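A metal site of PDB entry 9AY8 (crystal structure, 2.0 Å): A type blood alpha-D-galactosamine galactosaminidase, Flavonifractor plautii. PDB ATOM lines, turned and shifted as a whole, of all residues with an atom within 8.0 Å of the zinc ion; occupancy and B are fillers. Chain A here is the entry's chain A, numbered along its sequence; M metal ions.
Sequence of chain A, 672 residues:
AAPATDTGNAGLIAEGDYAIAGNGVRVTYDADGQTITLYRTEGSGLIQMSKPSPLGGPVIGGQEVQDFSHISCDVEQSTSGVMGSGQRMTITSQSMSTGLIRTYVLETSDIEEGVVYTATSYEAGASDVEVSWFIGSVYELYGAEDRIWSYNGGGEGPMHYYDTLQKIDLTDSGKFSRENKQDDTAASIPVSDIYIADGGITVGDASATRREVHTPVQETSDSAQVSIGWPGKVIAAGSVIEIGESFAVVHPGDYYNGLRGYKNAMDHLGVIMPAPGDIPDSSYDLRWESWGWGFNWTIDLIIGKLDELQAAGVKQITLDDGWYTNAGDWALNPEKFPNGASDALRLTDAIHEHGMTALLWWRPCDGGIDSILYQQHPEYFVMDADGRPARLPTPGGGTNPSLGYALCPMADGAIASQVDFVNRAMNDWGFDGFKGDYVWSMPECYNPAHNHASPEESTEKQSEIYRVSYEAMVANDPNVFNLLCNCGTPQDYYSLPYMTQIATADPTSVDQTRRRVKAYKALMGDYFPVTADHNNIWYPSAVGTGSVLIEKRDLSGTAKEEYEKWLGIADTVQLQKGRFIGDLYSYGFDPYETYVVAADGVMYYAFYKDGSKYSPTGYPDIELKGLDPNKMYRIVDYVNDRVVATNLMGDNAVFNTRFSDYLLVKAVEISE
A ring nitrogen (ND1) of His 452 is in hydrogen-bond range of the side-chain sulfur (SD) of Met 410 (3.5 Å).
The side-chain carboxylate (OE2) of Glu 457 sits at hydrogen-bond distance from a ring nitrogen (ND1) of His 452 (3.0 Å).
A ring nitrogen (NE2) of His 450 sits at hydrogen-bond distance from the backbone carbonyl oxygen (O) of Glu 379, 2.6 Å away.
The side-chain sulfur (SG) of Cys 445 sits close to the backbone NH (N) of Asn 447, at 3.6 Å.
The backbone NH of Cys 445 sits at hydrogen-bond distance from the side-chain hydroxyl of Ser 458.
N of Met 383 lies close to SG of Cys 445.
The side-chain sulfur of Cys 408 lies close to the backbone NH of Met 410, at 3.7 Å.
The backbone NH (N) of Cys 408 sits at hydrogen-bond distance from the backbone carbonyl oxygen (O) of Tyr 380 (2.9 Å).
Within 4 Å of the zinc ion: Cys 408, Cys 445, His 450 and His 452.
The zinc ion is bound by a ring nitrogen (NE2) of His 452 (2.0 Å), a ring nitrogen (ND1) of His 450 (2.1 Å), the side-chain sulfur (SG) of Cys 445 (2.3 Å) and the side-chain sulfur (SG) of Cys 408 (2.3 Å).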
ATOM      1  N   GLU A 379      14.253 -30.082  -5.536  1.00  0.00           N
ATOM      2  CA  GLU A 379      12.970 -29.766  -6.139  1.00  0.00           C
ATOM      3  C   GLU A 379      11.904 -30.778  -5.735  1.00  0.00           C
ATOM      4  O   GLU A 379      10.727 -30.493  -5.867  1.00  0.00           O
ATOM      5  CB  GLU A 379      13.082 -29.590  -7.669  1.00  0.00           C
ATOM      6  CG  GLU A 379      13.330 -30.865  -8.477  1.00  0.00           C
ATOM      7  CD  GLU A 379      14.784 -31.368  -8.540  1.00  0.00           C
ATOM      8  OE1 GLU A 379      15.042 -32.350  -9.284  1.00  0.00           O
ATOM      9  OE2 GLU A 379      15.650 -30.801  -7.823  1.00  0.00           O
ATOM     10  N   TYR A 380      12.297 -31.951  -5.208  1.00  0.00           N
ATOM     11  CA  TYR A 380      11.346 -32.964  -4.770  1.00  0.00           C
ATOM     12  C   TYR A 380      10.766 -32.643  -3.392  1.00  0.00           C
ATOM     13  O   TYR A 380       9.860 -33.348  -2.964  1.00  0.00           O
ATOM     14  CB  TYR A 380      11.953 -34.360  -4.673  1.00  0.00           C
ATOM     15  CG  TYR A 380      12.508 -34.991  -5.941  1.00  0.00           C
ATOM     16  CD1 TYR A 380      12.304 -34.421  -7.204  1.00  0.00           C
ATOM     17  CD2 TYR A 380      13.224 -36.178  -5.883  1.00  0.00           C
ATOM     18  CE1 TYR A 380      12.855 -34.990  -8.343  1.00  0.00           C
ATOM     19  CE2 TYR A 380      13.753 -36.765  -7.020  1.00  0.00           C
ATOM     20  CZ  TYR A 380      13.573 -36.165  -8.245  1.00  0.00           C
ATOM     21  OH  TYR A 380      14.115 -36.753  -9.347  1.00  0.00           O
ATOM     22  N   PHE A 381      11.278 -31.625  -2.703  1.00  0.00           N
ATOM     23  CA  PHE A 381      11.021 -31.431  -1.284  1.00  0.00           C
ATOM     24  C   PHE A 381      10.033 -30.299  -1.075  1.00  0.00           C
ATOM     25  O   PHE A 381       9.823 -29.472  -1.965  1.00  0.00           O
ATOM     26  CB  PHE A 381      12.324 -31.106  -0.550  1.00  0.00           C
ATOM     27  CG  PHE A 381      13.248 -32.303  -0.417  1.00  0.00           C
ATOM     28  CD1 PHE A 381      13.409 -32.959   0.792  1.00  0.00           C
ATOM     29  CD2 PHE A 381      13.916 -32.819  -1.518  1.00  0.00           C
ATOM     30  CE1 PHE A 381      14.247 -34.053   0.918  1.00  0.00           C
ATOM     31  CE2 PHE A 381      14.743 -33.923  -1.392  1.00  0.00           C
ATOM     32  CZ  PHE A 381      14.914 -34.536  -0.174  1.00  0.00           C
ATOM     33  N   VAL A 382       9.419 -30.288   0.111  1.00  0.00           N
ATOM     34  CA  VAL A 382       8.576 -29.166   0.502  1.00  0.00           C
ATOM     35  C   VAL A 382       9.487 -27.954   0.740  1.00  0.00           C
ATOM     36  O   VAL A 382      10.557 -28.075   1.322  1.00  0.00           O
ATOM     37  CB  VAL A 382       7.731 -29.470   1.750  1.00  0.00           C
ATOM     38  CG1 VAL A 382       6.952 -28.240   2.202  1.00  0.00           C
ATOM     39  CG2 VAL A 382       6.816 -30.663   1.536  1.00  0.00           C
ATOM     40  N   MET A 383       9.008 -26.795   0.276  1.00  0.00           N
ATOM     41  CA  MET A 383       9.700 -25.530   0.444  1.00  0.00           C
ATOM     42  C   MET A 383       8.811 -24.632   1.309  1.00  0.00           C
ATOM     43  O   MET A 383       7.596 -24.543   1.075  1.00  0.00           O
ATOM     44  CB  MET A 383       9.969 -24.883  -0.915  1.00  0.00           C
ATOM     45  CG  MET A 383      10.777 -23.602  -0.859  1.00  0.00           C
ATOM     46  SD  MET A 383      11.295 -23.016  -2.492  1.00  0.00           S
ATOM     47  CE  MET A 383      10.052 -21.730  -2.353  1.00  0.00           C
ATOM     48  N   ALA A 406      10.916 -32.687   4.521  1.00  0.00           N
ATOM     49  CA  ALA A 406       9.740 -33.310   3.956  1.00  0.00           C
ATOM     50  C   ALA A 406       9.838 -33.414   2.432  1.00  0.00           C
ATOM     51  O   ALA A 406      10.118 -32.441   1.771  1.00  0.00           O
ATOM     52  CB  ALA A 406       8.514 -32.524   4.353  1.00  0.00           C
ATOM     53  N   LEU A 407       9.529 -34.600   1.915  1.00  0.00           N
ATOM     54  CA  LEU A 407       9.241 -34.794   0.508  1.00  0.00           C
ATOM     55  C   LEU A 407       7.859 -34.230   0.188  1.00  0.00           C
ATOM     56  O   LEU A 407       6.887 -34.449   0.932  1.00  0.00           O
ATOM     57  CB  LEU A 407       9.295 -36.275   0.150  1.00  0.00           C
ATOM     58  CG  LEU A 407      10.684 -36.923   0.274  1.00  0.00           C
ATOM     59  CD1 LEU A 407      10.555 -38.430   0.201  1.00  0.00           C
ATOM     60  CD2 LEU A 407      11.605 -36.361  -0.800  1.00  0.00           C
ATOM     61  N   CYS A 408       7.772 -33.496  -0.915  1.00  0.00           N
ATOM     62  CA  CYS A 408       6.489 -32.973  -1.330  1.00  0.00           C
ATOM     63  C   CYS A 408       5.703 -34.104  -2.002  1.00  0.00           C
ATOM     64  O   CYS A 408       6.187 -34.684  -2.967  1.00  0.00           O
ATOM     65  CB  CYS A 408       6.618 -31.770  -2.249  1.00  0.00           C
ATOM     66  SG  CYS A 408       4.985 -31.172  -2.780  1.00  0.00           S
ATOM     67  N   PRO A 409       4.511 -34.437  -1.498  1.00  0.00           N
ATOM     68  CA  PRO A 409       3.783 -35.616  -1.970  1.00  0.00           C
ATOM     69  C   PRO A 409       3.248 -35.497  -3.402  1.00  0.00           C
ATOM     70  O   PRO A 409       2.784 -36.471  -3.968  1.00  0.00           O
ATOM     71  CB  PRO A 409       2.623 -35.766  -0.942  1.00  0.00           C
ATOM     72  CG  PRO A 409       2.443 -34.397  -0.346  1.00  0.00           C
ATOM     73  CD  PRO A 409       3.821 -33.730  -0.401  1.00  0.00           C
ATOM     74  N   MET A 410       3.283 -34.288  -3.966  1.00  0.00           N
ATOM     75  CA  MET A 410       2.880 -34.076  -5.329  1.00  0.00           C
ATOM     76  C   MET A 410       4.073 -34.046  -6.288  1.00  0.00           C
ATOM     77  O   MET A 410       3.887 -33.885  -7.474  1.00  0.00           O
ATOM     78  CB  MET A 410       2.094 -32.775  -5.418  1.00  0.00           C
ATOM     79  CG  MET A 410       0.663 -33.002  -4.824  1.00  0.00           C
ATOM     80  SD  MET A 410      -0.161 -31.415  -4.921  1.00  0.00           S
ATOM     81  CE  MET A 410      -0.260 -31.202  -6.708  1.00  0.00           C
ATOM     82  N   ALA A 411       5.288 -34.190  -5.767  1.00  0.00           N
ATOM     83  CA  ALA A 411       6.442 -34.193  -6.648  1.00  0.00           C
ATOM     84  C   ALA A 411       6.681 -35.639  -7.100  1.00  0.00           C
ATOM     85  O   ALA A 411       6.836 -36.539  -6.260  1.00  0.00           O
ATOM     86  CB  ALA A 411       7.657 -33.624  -5.939  1.00  0.00           C
ATOM     87  N   MET A 442       2.704 -33.015   7.610  1.00  0.00           N
ATOM     88  CA  MET A 442       3.375 -32.658   6.374  1.00  0.00           C
ATOM     89  C   MET A 442       3.263 -31.146   6.281  1.00  0.00           C
ATOM     90  O   MET A 442       2.164 -30.583   6.317  1.00  0.00           O
ATOM     91  CB  MET A 442       2.687 -33.322   5.178  1.00  0.00           C
ATOM     92  CG  MET A 442       3.075 -32.797   3.809  1.00  0.00           C
ATOM     93  SD  MET A 442       4.755 -33.208   3.318  1.00  0.00           S
ATOM     94  CE  MET A 442       4.734 -34.991   3.210  1.00  0.00           C
ATOM     95  N   PRO A 443       4.400 -30.418   6.169  1.00  0.00           N
ATOM     96  CA  PRO A 443       4.368 -28.963   6.121  1.00  0.00           C
ATOM     97  C   PRO A 443       3.785 -28.489   4.795  1.00  0.00           C
ATOM     98  O   PRO A 443       3.799 -29.208   3.796  1.00  0.00           O
ATOM     99  CB  PRO A 443       5.835 -28.561   6.324  1.00  0.00           C
ATOM    100  CG  PRO A 443       6.609 -29.764   5.754  1.00  0.00           C
ATOM    101  CD  PRO A 443       5.760 -30.980   6.055  1.00  0.00           C
ATOM    102  N   GLU A 444       3.305 -27.251   4.841  1.00  0.00           N
ATOM    103  CA  GLU A 444       2.777 -26.549   3.685  1.00  0.00           C
ATOM    104  C   GLU A 444       3.910 -26.238   2.726  1.00  0.00           C
ATOM    105  O   GLU A 444       5.017 -25.944   3.164  1.00  0.00           O
ATOM    106  CB  GLU A 444       2.125 -25.239   4.135  1.00  0.00           C
ATOM    107  CG  GLU A 444       0.895 -25.515   4.977  1.00  0.00           C
ATOM    108  CD  GLU A 444       0.073 -24.321   5.433  1.00  0.00           C
ATOM    109  OE1 GLU A 444      -1.033 -24.599   5.977  1.00  0.00           O
ATOM    110  OE2 GLU A 444       0.535 -23.177   5.307  1.00  0.00           O
ATOM    111  N   CYS A 445       3.585 -26.277   1.431  1.00  0.00           N
ATOM    112  CA  CYS A 445       4.593 -26.156   0.394  1.00  0.00           C
ATOM    113  C   CYS A 445       4.388 -24.887  -0.430  1.00  0.00           C
ATOM    114  O   CYS A 445       3.287 -24.655  -0.937  1.00  0.00           O
ATOM    115  CB  CYS A 445       4.620 -27.377  -0.518  1.00  0.00           C
ATOM    116  SG  CYS A 445       6.017 -27.311  -1.665  1.00  0.00           S
ATOM    117  N   TYR A 446       5.466 -24.100  -0.541  1.00  0.00           N
ATOM    118  CA  TYR A 446       5.434 -22.811  -1.209  1.00  0.00           C
ATOM    119  C   TYR A 446       6.363 -22.802  -2.427  1.00  0.00           C
ATOM    120  O   TYR A 446       6.689 -21.747  -2.946  1.00  0.00           O
ATOM    121  CB  TYR A 446       5.904 -21.714  -0.254  1.00  0.00           C
ATOM    122  CG  TYR A 446       4.904 -21.472   0.865  1.00  0.00           C
ATOM    123  CD1 TYR A 446       3.975 -20.431   0.772  1.00  0.00           C
ATOM    124  CD2 TYR A 446       4.885 -22.266   1.978  1.00  0.00           C
ATOM    125  CE1 TYR A 446       3.068 -20.202   1.785  1.00  0.00           C
ATOM    126  CE2 TYR A 446       3.976 -22.056   2.997  1.00  0.00           C
ATOM    127  CZ  TYR A 446       3.061 -21.012   2.885  1.00  0.00           C
ATOM    128  OH  TYR A 446       2.176 -20.786   3.893  1.00  0.00           O
ATOM    129  N   ASN A 447       6.790 -23.967  -2.894  1.00  0.00           N
ATOM    130  CA  ASN A 447       7.673 -23.985  -4.047  1.00  0.00           C
ATOM    131  C   ASN A 447       6.852 -23.603  -5.281  1.00  0.00           C
ATOM    132  O   ASN A 447       5.976 -24.334  -5.687  1.00  0.00           O
ATOM    133  CB  ASN A 447       8.310 -25.348  -4.235  1.00  0.00           C
ATOM    134  CG  ASN A 447       9.366 -25.288  -5.317  1.00  0.00           C
ATOM    135  OD1 ASN A 447       9.246 -24.497  -6.253  1.00  0.00           O
ATOM    136  ND2 ASN A 447      10.409 -26.097  -5.184  1.00  0.00           N
ATOM    137  N   PRO A 448       7.114 -22.440  -5.914  1.00  0.00           N
ATOM    138  CA  PRO A 448       6.317 -21.965  -7.045  1.00  0.00           C
ATOM    139  C   PRO A 448       6.322 -22.955  -8.201  1.00  0.00           C
ATOM    140  O   PRO A 448       5.313 -23.083  -8.880  1.00  0.00           O
ATOM    141  CB  PRO A 448       6.919 -20.612  -7.462  1.00  0.00           C
ATOM    142  CG  PRO A 448       7.790 -20.213  -6.311  1.00  0.00           C
ATOM    143  CD  PRO A 448       8.213 -21.512  -5.607  1.00  0.00           C
ATOM    144  N   ALA A 449       7.419 -23.706  -8.367  1.00  0.00           N
ATOM    145  CA  ALA A 449       7.547 -24.648  -9.462  1.00  0.00           C
ATOM    146  C   ALA A 449       6.581 -25.820  -9.328  1.00  0.00           C
ATOM    147  O   ALA A 449       6.265 -26.508 -10.305  1.00  0.00           O
ATOM    148  CB  ALA A 449       8.988 -25.128  -9.556  1.00  0.00           C
ATOM    149  N   HIS A 450       6.128 -26.085  -8.091  1.00  0.00           N
ATOM    150  CA  HIS A 450       5.183 -27.170  -7.843  1.00  0.00           C
ATOM    151  C   HIS A 450       3.772 -26.734  -8.243  1.00  0.00           C
ATOM    152  O   HIS A 450       2.909 -27.591  -8.346  1.00  0.00           O
ATOM    153  CB  HIS A 450       5.215 -27.612  -6.367  1.00  0.00           C
ATOM    154  CG  HIS A 450       6.504 -28.242  -5.957  1.00  0.00           C
ATOM    155  ND1 HIS A 450       6.742 -28.731  -4.693  1.00  0.00           N
ATOM    156  CD2 HIS A 450       7.664 -28.409  -6.652  1.00  0.00           C
ATOM    157  CE1 HIS A 450       7.967 -29.236  -4.638  1.00  0.00           C
ATOM    158  NE2 HIS A 450       8.546 -29.037  -5.806  1.00  0.00           N
ATOM    159  N   ASN A 451       3.519 -25.425  -8.392  1.00  0.00           N
ATOM    160  CA  ASN A 451       2.223 -24.933  -8.843  1.00  0.00           C
ATOM    161  C   ASN A 451       1.079 -25.449  -7.967  1.00  0.00           C
ATOM    162  O   ASN A 451       0.062 -25.892  -8.476  1.00  0.00           O
ATOM    163  CB  ASN A 451       1.960 -25.305 -10.303  1.00  0.00           C
ATOM    164  CG  ASN A 451       2.860 -24.504 -11.226  1.00  0.00           C
ATOM    165  OD1 ASN A 451       2.763 -23.278 -11.252  1.00  0.00           O
ATOM    166  ND2 ASN A 451       3.760 -25.156 -11.947  1.00  0.00           N
ATOM    167  N   HIS A 452       1.223 -25.400  -6.635  1.00  0.00           N
ATOM    168  CA  HIS A 452       0.173 -25.898  -5.769  1.00  0.00           C
ATOM    169  C   HIS A 452      -1.083 -25.028  -5.846  1.00  0.00           C
ATOM    170  O   HIS A 452      -1.009 -23.817  -5.962  1.00  0.00           O
ATOM    171  CB  HIS A 452       0.676 -26.022  -4.330  1.00  0.00           C
ATOM    172  CG  HIS A 452       1.715 -27.072  -4.127  1.00  0.00           C
ATOM    173  ND1 HIS A 452       1.401 -28.410  -4.164  1.00  0.00           N
ATOM    174  CD2 HIS A 452       3.052 -26.981  -3.855  1.00  0.00           C
ATOM    175  CE1 HIS A 452       2.502 -29.108  -3.896  1.00  0.00           C
ATOM    176  NE2 HIS A 452       3.538 -28.259  -3.693  1.00  0.00           N
ATOM    177  N   SER A 454      -2.924 -24.496  -3.335  1.00  0.00           N
ATOM    178  CA  SER A 454      -2.755 -23.706  -2.120  1.00  0.00           C
ATOM    179  C   SER A 454      -1.573 -24.285  -1.383  1.00  0.00           C
ATOM    180  O   SER A 454      -1.200 -25.427  -1.633  1.00  0.00           O
ATOM    181  CB  SER A 454      -3.996 -23.797  -1.235  1.00  0.00           C
ATOM    182  OG  SER A 454      -4.119 -25.139  -0.719  1.00  0.00           O
ATOM    183  N   PRO A 455      -0.945 -23.574  -0.428  1.00  0.00           N
ATOM    184  CA  PRO A 455       0.146 -24.150   0.354  1.00  0.00           C
ATOM    185  C   PRO A 455      -0.246 -25.382   1.157  1.00  0.00           C
ATOM    186  O   PRO A 455       0.576 -26.261   1.357  1.00  0.00           O
ATOM    187  CB  PRO A 455       0.578 -22.969   1.262  1.00  0.00           C
ATOM    188  CG  PRO A 455       0.104 -21.738   0.495  1.00  0.00           C
ATOM    189  CD  PRO A 455      -1.213 -22.155  -0.135  1.00  0.00           C
ATOM    190  N   GLU A 457      -1.980 -27.776   0.171  1.00  0.00           N
ATOM    191  CA  GLU A 457      -2.116 -28.941  -0.685  1.00  0.00           C
ATOM    192  C   GLU A 457      -1.127 -30.056  -0.308  1.00  0.00           C
ATOM    193  O   GLU A 457      -1.460 -31.229  -0.362  1.00  0.00           O
ATOM    194  CB  GLU A 457      -1.980 -28.465  -2.129  1.00  0.00           C
ATOM    195  CG  GLU A 457      -2.332 -29.572  -3.111  1.00  0.00           C
ATOM    196  CD  GLU A 457      -2.331 -29.145  -4.554  1.00  0.00           C
ATOM    197  OE1 GLU A 457      -3.283 -29.560  -5.221  1.00  0.00           O
ATOM    198  OE2 GLU A 457      -1.440 -28.391  -5.001  1.00  0.00           O
ATOM    199  N   SER A 458       0.108 -29.700   0.069  1.00  0.00           N
ATOM    200  CA  SER A 458       1.078 -30.714   0.461  1.00  0.00           C
ATOM    201  C   SER A 458       0.531 -31.487   1.658  1.00  0.00           C
ATOM    202  O   SER A 458       0.501 -32.708   1.657  1.00  0.00           O
ATOM    203  CB  SER A 458       2.403 -30.088   0.753  1.00  0.00           C
ATOM    204  OG  SER A 458       2.280 -28.967   1.616  1.00  0.00           O
HETATM  205 ZN    ZN M   1       5.333 -28.901  -3.116  1.00  0.00          ZN
